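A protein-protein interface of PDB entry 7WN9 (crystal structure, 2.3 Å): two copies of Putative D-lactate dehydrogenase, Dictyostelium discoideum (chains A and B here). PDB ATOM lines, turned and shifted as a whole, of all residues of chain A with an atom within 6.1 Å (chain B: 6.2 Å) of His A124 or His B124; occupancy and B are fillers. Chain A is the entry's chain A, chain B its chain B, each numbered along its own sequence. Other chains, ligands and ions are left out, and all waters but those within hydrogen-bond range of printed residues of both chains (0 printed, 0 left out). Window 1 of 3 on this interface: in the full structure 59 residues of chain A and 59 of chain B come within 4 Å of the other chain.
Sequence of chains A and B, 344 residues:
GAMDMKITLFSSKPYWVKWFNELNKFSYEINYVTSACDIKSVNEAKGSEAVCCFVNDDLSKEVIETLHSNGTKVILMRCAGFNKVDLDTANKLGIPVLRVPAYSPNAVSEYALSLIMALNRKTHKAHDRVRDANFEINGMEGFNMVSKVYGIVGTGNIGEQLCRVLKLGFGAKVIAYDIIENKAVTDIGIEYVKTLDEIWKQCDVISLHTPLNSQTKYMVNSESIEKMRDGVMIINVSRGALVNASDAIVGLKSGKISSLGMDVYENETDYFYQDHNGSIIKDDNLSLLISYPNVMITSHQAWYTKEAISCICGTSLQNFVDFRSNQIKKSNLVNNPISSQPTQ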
ATOM      1  N   ALA A 118     -19.568 -27.707  23.219  1.00  0.00           N
ATOM      2  CA  ALA A 118     -18.819 -27.247  24.377  1.00  0.00           C
ATOM      3  C   ALA A 118     -17.454 -27.918  24.437  1.00  0.00           C
ATOM      4  O   ALA A 118     -16.433 -27.248  24.614  1.00  0.00           O
ATOM      5  CB  ALA A 118     -19.615 -27.512  25.662  1.00  0.00           C
ATOM      6  N   LEU A 119     -17.417 -29.253  24.322  1.00  0.00           N
ATOM      7  CA  LEU A 119     -16.131 -29.945  24.393  1.00  0.00           C
ATOM      8  C   LEU A 119     -15.274 -29.677  23.168  1.00  0.00           C
ATOM      9  O   LEU A 119     -14.052 -29.824  23.230  1.00  0.00           O
ATOM     10  CB  LEU A 119     -16.333 -31.449  24.541  1.00  0.00           C
ATOM     11  CG  LEU A 119     -17.039 -31.905  25.818  1.00  0.00           C
ATOM     12  CD1 LEU A 119     -17.444 -33.362  25.678  1.00  0.00           C
ATOM     13  CD2 LEU A 119     -16.153 -31.705  27.058  1.00  0.00           C
ATOM     14  N   ARG A 121     -15.404 -26.578  20.949  1.00  0.00           N
ATOM     15  CA  ARG A 121     -14.938 -25.196  20.940  1.00  0.00           C
ATOM     16  C   ARG A 121     -14.607 -24.654  22.330  1.00  0.00           C
ATOM     17  O   ARG A 121     -14.030 -23.567  22.423  1.00  0.00           O
ATOM     18  CB  ARG A 121     -15.976 -24.299  20.247  1.00  0.00           C
ATOM     19  CG  ARG A 121     -16.359 -24.788  18.817  1.00  0.00           C
ATOM     20  CD  ARG A 121     -15.112 -25.071  17.929  1.00  0.00           C
ATOM     21  NE  ARG A 121     -14.267 -23.884  17.802  1.00  0.00           N
ATOM     22  CZ  ARG A 121     -14.405 -22.973  16.837  1.00  0.00           C
ATOM     23  NH1 ARG A 121     -13.630 -21.906  16.812  1.00  0.00           N
ATOM     24  NH2 ARG A 121     -15.331 -23.123  15.902  1.00  0.00           N
ATOM     25  N   LYS A 122     -14.950 -25.375  23.399  1.00  0.00           N
ATOM     26  CA  LYS A 122     -14.498 -25.052  24.763  1.00  0.00           C
ATOM     27  C   LYS A 122     -14.985 -23.683  25.240  1.00  0.00           C
ATOM     28  O   LYS A 122     -14.264 -22.950  25.925  1.00  0.00           O
ATOM     29  CB  LYS A 122     -12.972 -25.157  24.856  1.00  0.00           C
ATOM     30  CG  LYS A 122     -12.516 -26.514  24.380  1.00  0.00           C
ATOM     31  CD  LYS A 122     -11.059 -26.755  24.533  1.00  0.00           C
ATOM     32  CE  LYS A 122     -10.721 -28.095  23.921  1.00  0.00           C
ATOM     33  NZ  LYS A 122     -11.244 -28.160  22.528  1.00  0.00           N
ATOM     34  N   THR A 123     -16.224 -23.339  24.890  1.00  0.00           N
ATOM     35  CA  THR A 123     -16.792 -22.076  25.349  1.00  0.00           C
ATOM     36  C   THR A 123     -16.806 -21.977  26.869  1.00  0.00           C
ATOM     37  O   THR A 123     -16.642 -20.880  27.412  1.00  0.00           O
ATOM     38  CB  THR A 123     -18.208 -21.902  24.803  1.00  0.00           C
ATOM     39  OG1 THR A 123     -18.943 -23.104  25.051  1.00  0.00           O
ATOM     40  CG2 THR A 123     -18.197 -21.603  23.272  1.00  0.00           C
ATOM     41  N   HIS A 124     -16.998 -23.094  27.581  1.00  0.00           N
ATOM     42  CA  HIS A 124     -17.034 -23.025  29.048  1.00  0.00           C
ATOM     43  C   HIS A 124     -15.643 -22.768  29.631  1.00  0.00           C
ATOM     44  O   HIS A 124     -15.501 -22.030  30.613  1.00  0.00           O
ATOM     45  CB  HIS A 124     -17.629 -24.309  29.624  1.00  0.00           C
ATOM     46  CG  HIS A 124     -16.900 -25.545  29.208  1.00  0.00           C
ATOM     47  ND1 HIS A 124     -16.822 -25.952  27.893  1.00  0.00           N
ATOM     48  CD2 HIS A 124     -16.203 -26.459  29.927  1.00  0.00           C
ATOM     49  CE1 HIS A 124     -16.101 -27.058  27.818  1.00  0.00           C
ATOM     50  NE2 HIS A 124     -15.713 -27.386  29.038  1.00  0.00           N
ATOM     51  N   LYS A 125     -14.609 -23.356  29.032  1.00  0.00           N
ATOM     52  CA  LYS A 125     -13.232 -23.057  29.419  1.00  0.00           C
ATOM     53  C   LYS A 125     -12.870 -21.606  29.115  1.00  0.00           C
ATOM     54  O   LYS A 125     -12.188 -20.943  29.912  1.00  0.00           O
ATOM     55  CB  LYS A 125     -12.277 -24.005  28.690  1.00  0.00           C
ATOM     56  CG  LYS A 125     -10.800 -23.847  29.065  1.00  0.00           C
ATOM     57  CD  LYS A 125      -9.907 -24.790  28.242  1.00  0.00           C
ATOM     58  CE  LYS A 125      -8.545 -25.027  28.917  1.00  0.00           C
ATOM     59  NZ  LYS A 125      -8.596 -25.961  30.110  1.00  0.00           N
ATOM     60  N   ALA A 126     -13.305 -21.100  27.962  1.00  0.00           N
ATOM     61  CA  ALA A 126     -13.049 -19.703  27.641  1.00  0.00           C
ATOM     62  C   ALA A 126     -13.755 -18.793  28.634  1.00  0.00           C
ATOM     63  O   ALA A 126     -13.185 -17.792  29.089  1.00  0.00           O
ATOM     64  CB  ALA A 126     -13.505 -19.403  26.209  1.00  0.00           C
ATOM     65  N   HIS A 127     -14.998 -19.137  28.991  1.00  0.00           N
ATOM     66  CA  HIS A 127     -15.755 -18.339  29.951  1.00  0.00           C
ATOM     67  C   HIS A 127     -15.042 -18.273  31.296  1.00  0.00           C
ATOM     68  O   HIS A 127     -14.924 -17.195  31.889  1.00  0.00           O
ATOM     69  CB  HIS A 127     -17.170 -18.913  30.111  1.00  0.00           C
ATOM     70  CG  HIS A 127     -18.023 -18.168  31.091  1.00  0.00           C
ATOM     71  ND1 HIS A 127     -18.523 -16.907  30.838  1.00  0.00           N
ATOM     72  CD2 HIS A 127     -18.460 -18.503  32.329  1.00  0.00           C
ATOM     73  CE1 HIS A 127     -19.233 -16.499  31.873  1.00  0.00           C
ATOM     74  NE2 HIS A 127     -19.215 -17.451  32.790  1.00  0.00           N
ATOM     75  N   ASP A 128     -14.533 -19.407  31.780  1.00  0.00           N
ATOM     76  CA  ASP A 128     -13.832 -19.391  33.062  1.00  0.00           C
ATOM     77  C   ASP A 128     -12.542 -18.586  32.977  1.00  0.00           C
ATOM     78  O   ASP A 128     -12.201 -17.853  33.910  1.00  0.00           O
ATOM     79  CB  ASP A 128     -13.554 -20.821  33.534  1.00  0.00           C
ATOM     80  CG  ASP A 128     -14.842 -21.605  33.808  1.00  0.00           C
ATOM     81  OD1 ASP A 128     -15.900 -20.964  34.031  1.00  0.00           O
ATOM     82  OD2 ASP A 128     -14.793 -22.856  33.786  1.00  0.00           O
ATOM     83  N   ARG A 129     -11.814 -18.691  31.865  1.00  0.00           N
ATOM     84  CA  ARG A 129     -10.597 -17.894  31.728  1.00  0.00           C
ATOM     85  C   ARG A 129     -10.913 -16.405  31.726  1.00  0.00           C
ATOM     86  O   ARG A 129     -10.281 -15.621  32.443  1.00  0.00           O
ATOM     87  CB  ARG A 129      -9.849 -18.275  30.455  1.00  0.00           C
ATOM     88  CG  ARG A 129      -9.030 -19.564  30.567  1.00  0.00           C
ATOM     89  CD  ARG A 129      -8.105 -19.713  29.352  1.00  0.00           C
ATOM     90  NE  ARG A 129      -7.465 -21.024  29.348  1.00  0.00           N
ATOM     91  CZ  ARG A 129      -6.690 -21.487  28.375  1.00  0.00           C
ATOM     92  NH1 ARG A 129      -6.445 -20.748  27.295  1.00  0.00           N
ATOM     93  NH2 ARG A 129      -6.162 -22.695  28.482  1.00  0.00           N
ATOM     94  N   PRO A 293     -10.376 -31.588  33.073  1.00  0.00           N
ATOM     95  CA  PRO A 293     -10.623 -30.420  32.215  1.00  0.00           C
ATOM     96  C   PRO A 293     -11.360 -30.751  30.927  1.00  0.00           C
ATOM     97  O   PRO A 293     -11.957 -29.842  30.338  1.00  0.00           O
ATOM     98  CB  PRO A 293      -9.208 -29.896  31.926  1.00  0.00           C
ATOM     99  CG  PRO A 293      -8.334 -31.114  32.075  1.00  0.00           C
ATOM    100  CD  PRO A 293      -8.945 -31.897  33.197  1.00  0.00           C
ATOM    101  N   VAL A 295     -13.886 -33.028  30.575  1.00  0.00           N
ATOM    102  CA  VAL A 295     -15.072 -33.785  30.939  1.00  0.00           C
ATOM    103  C   VAL A 295     -16.174 -32.823  31.335  1.00  0.00           C
ATOM    104  O   VAL A 295     -15.936 -31.843  32.050  1.00  0.00           O
ATOM    105  CB  VAL A 295     -14.811 -34.771  32.097  1.00  0.00           C
ATOM    106  CG1 VAL A 295     -16.120 -35.420  32.523  1.00  0.00           C
ATOM    107  CG2 VAL A 295     -13.790 -35.811  31.683  1.00  0.00           C
ATOM    108  N   MET A 296     -17.385 -33.115  30.875  1.00  0.00           N
ATOM    109  CA  MET A 296     -18.580 -32.386  31.271  1.00  0.00           C
ATOM    110  C   MET A 296     -19.581 -33.384  31.838  1.00  0.00           C
ATOM    111  O   MET A 296     -19.984 -34.326  31.144  1.00  0.00           O
ATOM    112  CB  MET A 296     -19.183 -31.624  30.087  1.00  0.00           C
ATOM    113  CG  MET A 296     -18.380 -30.381  29.671  1.00  0.00           C
ATOM    114  SD  MET A 296     -19.141 -28.833  30.231  1.00  0.00           S
ATOM    115  CE  MET A 296     -20.727 -28.938  29.423  1.00  0.00           C
ATOM    116  N   MET B 117     -25.808 -21.988  21.515  1.00  0.00           N
ATOM    117  CA  MET B 117     -26.086 -23.176  22.313  1.00  0.00           C
ATOM    118  C   MET B 117     -25.707 -22.954  23.770  1.00  0.00           C
ATOM    119  O   MET B 117     -26.454 -23.328  24.678  1.00  0.00           O
ATOM    120  CB  MET B 117     -25.338 -24.384  21.742  1.00  0.00           C
ATOM    121  CG  MET B 117     -25.746 -24.761  20.333  1.00  0.00           C
ATOM    122  SD  MET B 117     -27.510 -24.533  20.010  1.00  0.00           S
ATOM    123  CE  MET B 117     -28.217 -25.842  21.017  1.00  0.00           C
ATOM    124  N   ALA B 118     -24.554 -22.326  24.010  1.00  0.00           N
ATOM    125  CA  ALA B 118     -24.112 -22.102  25.376  1.00  0.00           C
ATOM    126  C   ALA B 118     -25.089 -21.207  26.118  1.00  0.00           C
ATOM    127  O   ALA B 118     -25.495 -21.518  27.239  1.00  0.00           O
ATOM    128  CB  ALA B 118     -22.707 -21.494  25.397  1.00  0.00           C
ATOM    129  N   LEU B 119     -25.475 -20.084  25.506  1.00  0.00           N
ATOM    130  CA  LEU B 119     -26.422 -19.176  26.160  1.00  0.00           C
ATOM    131  C   LEU B 119     -27.808 -19.793  26.285  1.00  0.00           C
ATOM    132  O   LEU B 119     -28.556 -19.451  27.202  1.00  0.00           O
ATOM    133  CB  LEU B 119     -26.524 -17.859  25.392  1.00  0.00           C
ATOM    134  CG  LEU B 119     -25.236 -17.032  25.412  1.00  0.00           C
ATOM    135  CD1 LEU B 119     -25.317 -15.906  24.396  1.00  0.00           C
ATOM    136  CD2 LEU B 119     -25.002 -16.475  26.819  1.00  0.00           C
ATOM    137  N   ASN B 120     -28.175 -20.674  25.361  1.00  0.00           N
ATOM    138  CA  ASN B 120     -29.463 -21.349  25.379  1.00  0.00           C
ATOM    139  C   ASN B 120     -29.480 -22.434  26.463  1.00  0.00           C
ATOM    140  O   ASN B 120     -30.182 -22.299  27.469  1.00  0.00           O
ATOM    141  CB  ASN B 120     -29.744 -21.907  23.976  1.00  0.00           C
ATOM    142  CG  ASN B 120     -30.974 -22.810  23.913  1.00  0.00           C
ATOM    143  OD1 ASN B 120     -31.674 -22.996  24.895  1.00  0.00           O
ATOM    144  ND2 ASN B 120     -31.227 -23.381  22.731  1.00  0.00           N
ATOM    145  N   ARG B 121     -28.687 -23.485  26.298  1.00  0.00           N
ATOM    146  CA  ARG B 121     -28.723 -24.623  27.208  1.00  0.00           C
ATOM    147  C   ARG B 121     -27.822 -24.449  28.430  1.00  0.00           C
ATOM    148  O   ARG B 121     -27.896 -25.266  29.356  1.00  0.00           O
ATOM    149  CB  ARG B 121     -28.352 -25.910  26.448  1.00  0.00           C
ATOM    150  CG  ARG B 121     -29.197 -26.138  25.169  1.00  0.00           C
ATOM    151  CD  ARG B 121     -30.716 -26.037  25.427  1.00  0.00           C
ATOM    152  NE  ARG B 121     -31.130 -26.962  26.483  1.00  0.00           N
ATOM    153  CZ  ARG B 121     -31.568 -28.208  26.278  1.00  0.00           C
ATOM    154  NH1 ARG B 121     -31.889 -28.969  27.304  1.00  0.00           N
ATOM    155  NH2 ARG B 121     -31.673 -28.700  25.051  1.00  0.00           N
ATOM    156  N   LYS B 122     -26.963 -23.425  28.439  1.00  0.00           N
ATOM    157  CA  LYS B 122     -26.210 -23.011  29.631  1.00  0.00           C
ATOM    158  C   LYS B 122     -25.267 -24.098  30.147  1.00  0.00           C
ATOM    159  O   LYS B 122     -25.136 -24.311  31.355  1.00  0.00           O
ATOM    160  CB  LYS B 122     -27.171 -22.552  30.730  1.00  0.00           C
ATOM    161  CG  LYS B 122     -27.974 -21.331  30.302  1.00  0.00           C
ATOM    162  CD  LYS B 122     -29.094 -21.014  31.250  1.00  0.00           C
ATOM    163  CE  LYS B 122     -29.988 -19.947  30.666  1.00  0.00           C
ATOM    164  NZ  LYS B 122     -30.680 -20.454  29.439  1.00  0.00           N
ATOM    165  N   THR B 123     -24.580 -24.777  29.228  1.00  0.00           N
ATOM    166  CA  THR B 123     -23.628 -25.808  29.638  1.00  0.00           C
ATOM    167  C   THR B 123     -22.509 -25.241  30.504  1.00  0.00           C
ATOM    168  O   THR B 123     -22.016 -25.935  31.400  1.00  0.00           O
ATOM    169  CB  THR B 123     -23.040 -26.498  28.406  1.00  0.00           C
ATOM    170  OG1 THR B 123     -22.727 -25.497  27.425  1.00  0.00           O
ATOM    171  CG2 THR B 123     -24.044 -27.525  27.810  1.00  0.00           C
ATOM    172  N   HIS B 124     -22.076 -24.000  30.245  1.00  0.00           N
ATOM    173  CA  HIS B 124     -21.018 -23.399  31.059  1.00  0.00           C
ATOM    174  C   HIS B 124     -21.501 -23.104  32.478  1.00  0.00           C
ATOM    175  O   HIS B 124     -20.746 -23.266  33.443  1.00  0.00           O
ATOM    176  CB  HIS B 124     -20.511 -22.123  30.393  1.00  0.00           C
ATOM    177  CG  HIS B 124     -21.595 -21.147  30.073  1.00  0.00           C
ATOM    178  ND1 HIS B 124     -22.661 -21.465  29.261  1.00  0.00           N
ATOM    179  CD2 HIS B 124     -21.789 -19.862  30.463  1.00  0.00           C
ATOM    180  CE1 HIS B 124     -23.466 -20.421  29.164  1.00  0.00           C
ATOM    181  NE2 HIS B 124     -22.963 -19.437  29.888  1.00  0.00           N
ATOM    182  N   LYS B 125     -22.755 -22.676  32.624  1.00  0.00           N
ATOM    183  CA  LYS B 125     -23.329 -22.466  33.952  1.00  0.00           C
ATOM    184  C   LYS B 125     -23.475 -23.785  34.709  1.00  0.00           C
ATOM    185  O   LYS B 125     -23.207 -23.853  35.917  1.00  0.00           O
ATOM    186  CB  LYS B 125     -24.683 -21.760  33.819  1.00  0.00           C
ATOM    187  CG  LYS B 125     -25.303 -21.301  35.142  1.00  0.00           C
ATOM    188  CD  LYS B 125     -26.643 -20.561  34.932  1.00  0.00           C
ATOM    189  CE  LYS B 125     -27.101 -19.850  36.213  1.00  0.00           C
ATOM    190  NZ  LYS B 125     -26.259 -18.640  36.550  1.00  0.00           N
ATOM    191  N   ALA B 126     -23.885 -24.847  34.015  1.00  0.00           N
ATOM    192  CA  ALA B 126     -24.000 -26.150  34.664  1.00  0.00           C
ATOM    193  C   ALA B 126     -22.627 -26.696  35.038  1.00  0.00           C
ATOM    194  O   ALA B 126     -22.463 -27.319  36.090  1.00  0.00           O
ATOM    195  CB  ALA B 126     -24.743 -27.134  33.748  1.00  0.00           C
ATOM    196  N   HIS B 127     -21.629 -26.464  34.185  1.00  0.00           N
ATOM    197  CA  HIS B 127     -20.275 -26.910  34.485  1.00  0.00           C
ATOM    198  C   HIS B 127     -19.751 -26.253  35.759  1.00  0.00           C
ATOM    199  O   HIS B 127     -19.188 -26.924  36.630  1.00  0.00           O
ATOM    200  CB  HIS B 127     -19.354 -26.616  33.296  1.00  0.00           C
ATOM    201  CG  HIS B 127     -17.930 -27.009  33.524  1.00  0.00           C
ATOM    202  ND1 HIS B 127     -17.513 -28.323  33.536  1.00  0.00           N
ATOM    203  CD2 HIS B 127     -16.828 -26.262  33.770  1.00  0.00           C
ATOM    204  CE1 HIS B 127     -16.213 -28.369  33.764  1.00  0.00           C
ATOM    205  NE2 HIS B 127     -15.773 -27.132  33.905  1.00  0.00           N
ATOM    206  N   ASP B 128     -19.934 -24.938  35.890  1.00  0.00           N
ATOM    207  CA  ASP B 128     -19.489 -24.257  37.103  1.00  0.00           C
ATOM    208  C   ASP B 128     -20.251 -24.737  38.337  1.00  0.00           C
ATOM    209  O   ASP B 128     -19.662 -24.890  39.409  1.00  0.00           O
ATOM    210  CB  ASP B 128     -19.626 -22.740  36.934  1.00  0.00           C
ATOM    211  CG  ASP B 128     -18.712 -22.203  35.839  1.00  0.00           C
ATOM    212  OD1 ASP B 128     -17.724 -22.903  35.494  1.00  0.00           O
ATOM    213  OD2 ASP B 128     -18.985 -21.100  35.319  1.00  0.00           O
ATOM    214  N   ARG B 129     -21.556 -24.970  38.224  1.00  0.00           N
ATOM    215  CA  ARG B 129     -22.290 -25.464  39.389  1.00  0.00           C
ATOM    216  C   ARG B 129     -21.794 -26.839  39.807  1.00  0.00           C
ATOM    217  O   ARG B 129     -21.533 -27.090  40.994  1.00  0.00           O
ATOM    218  CB  ARG B 129     -23.788 -25.515  39.104  1.00  0.00           C
ATOM    219  CG  ARG B 129     -24.483 -24.181  39.201  1.00  0.00           C
ATOM    220  CD  ARG B 129     -25.988 -24.376  39.053  1.00  0.00           C
ATOM    221  NE  ARG B 129     -26.689 -23.097  38.986  1.00  0.00           N
ATOM    222  CZ  ARG B 129     -28.007 -22.973  38.893  1.00  0.00           C
ATOM    223  NH1 ARG B 129     -28.785 -24.057  38.855  1.00  0.00           N
ATOM    224  NH2 ARG B 129     -28.547 -21.765  38.835  1.00  0.00           N
ATOM    225  N   PRO B 293     -24.219 -12.847  34.286  1.00  0.00           N
ATOM    226  CA  PRO B 293     -24.441 -14.297  34.149  1.00  0.00           C
ATOM    227  C   PRO B 293     -24.976 -14.719  32.791  1.00  0.00           C
ATOM    228  O   PRO B 293     -24.873 -15.905  32.451  1.00  0.00           O
ATOM    229  CB  PRO B 293     -25.462 -14.601  35.258  1.00  0.00           C
ATOM    230  CG  PRO B 293     -26.194 -13.312  35.447  1.00  0.00           C
ATOM    231  CD  PRO B 293     -25.153 -12.231  35.240  1.00  0.00           C
ATOM    232  N   VAL B 295     -24.043 -13.354  29.793  1.00  0.00           N
ATOM    233  CA  VAL B 295     -23.151 -12.775  28.801  1.00  0.00           C
ATOM    234  C   VAL B 295     -21.948 -13.688  28.639  1.00  0.00           C
ATOM    235  O   VAL B 295     -21.382 -14.169  29.626  1.00  0.00           O
ATOM    236  CB  VAL B 295     -22.686 -11.354  29.191  1.00  0.00           C
ATOM    237  CG1 VAL B 295     -21.618 -10.853  28.213  1.00  0.00           C
ATOM    238  CG2 VAL B 295     -23.857 -10.401  29.233  1.00  0.00           C
ATOM    239  N   MET B 296     -21.562 -13.929  27.388  1.00  0.00           N
ATOM    240  CA  MET B 296     -20.326 -14.628  27.058  1.00  0.00           C
ATOM    241  C   MET B 296     -19.467 -13.701  26.215  1.00  0.00           C
ATOM    242  O   MET B 296     -19.917 -13.224  25.165  1.00  0.00           O
ATOM    243  CB  MET B 296     -20.609 -15.920  26.297  1.00  0.00           C
ATOM    244  CG  MET B 296     -21.203 -17.006  27.160  1.00  0.00           C
ATOM    245  SD  MET B 296     -19.949 -18.217  27.584  1.00  0.00           S
ATOM    246  CE  MET B 296     -19.609 -18.903  25.974  1.00  0.00           C
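The side-chain sulfur (SD) of Met A296 sits at hydrogen-bond distance from a ring nitrogen (ND1) of His B127 (3.7 Å).
ND1 of His A127 sits at hydrogen-bond distance from SD of Met B296.
The side-chain carboxylate (OD1) of Asp A128 lies close to the side-chain carboxylate (OD1) of Asp B128, at 3.0 Å.
O of Ala B118 lies close to ND1 of His B124, at 3.5 Å.
Among the printed residues, merely in contact across the chains: Thr A123 with Met B296 (3.5 Å), Met A296 with Thr B123 (3.5 Å), His A124 with His B124 (3.7 Å), Val A295 with His B127 (3.9 Å), His A127 with Val B295 (3.9 Å), His A124 with His B127 (3.9 Å), Asp A128 with His B127 (3.97 Å) and His A127 with Asp B128 (3.995 Å).
His A124 touches two residues of chain B.
His B124 touches one residue of chain A.
Printed residues of chain B within 4 Å of His A127: Asp B128, Val B295 and Met B296.
Of the printed residues of chain A, His B127 touches His A124 (3.9 Å), Asp A128 (3.97 Å), Val A295 (3.9 Å) and Met A296 (3.7 Å).
Of the printed residues of chain B, Asp A128 touches His B127 and Asp B128.
The nearest printed residue of chain A that does not touch Met B296 is His A124 (5.2 Å).
Along chain A the printed residues that touch a printed residue of chain B span positions 123 to 296.
Of the 16 printed residues of chain B, 6 touch a printed residue of chain A.
Among the printed residues, 11 pairs touch across the chains.
Among the printed residues, no Asp or Glu carboxylate lies within 4 Å of a Lys or Arg side-chain nitrogen of the other chain.
Thr A123 touches Met B296, and with the chains exchanged Met A296 touches Thr B123.
His B124 touches its own counterpart, His A124.
His A127 touches Met B296, and with the chains exchanged Met A296 touches His B127.
Asp A128 touches its own counterpart, Asp B128.
14 positions are printed for both chains.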
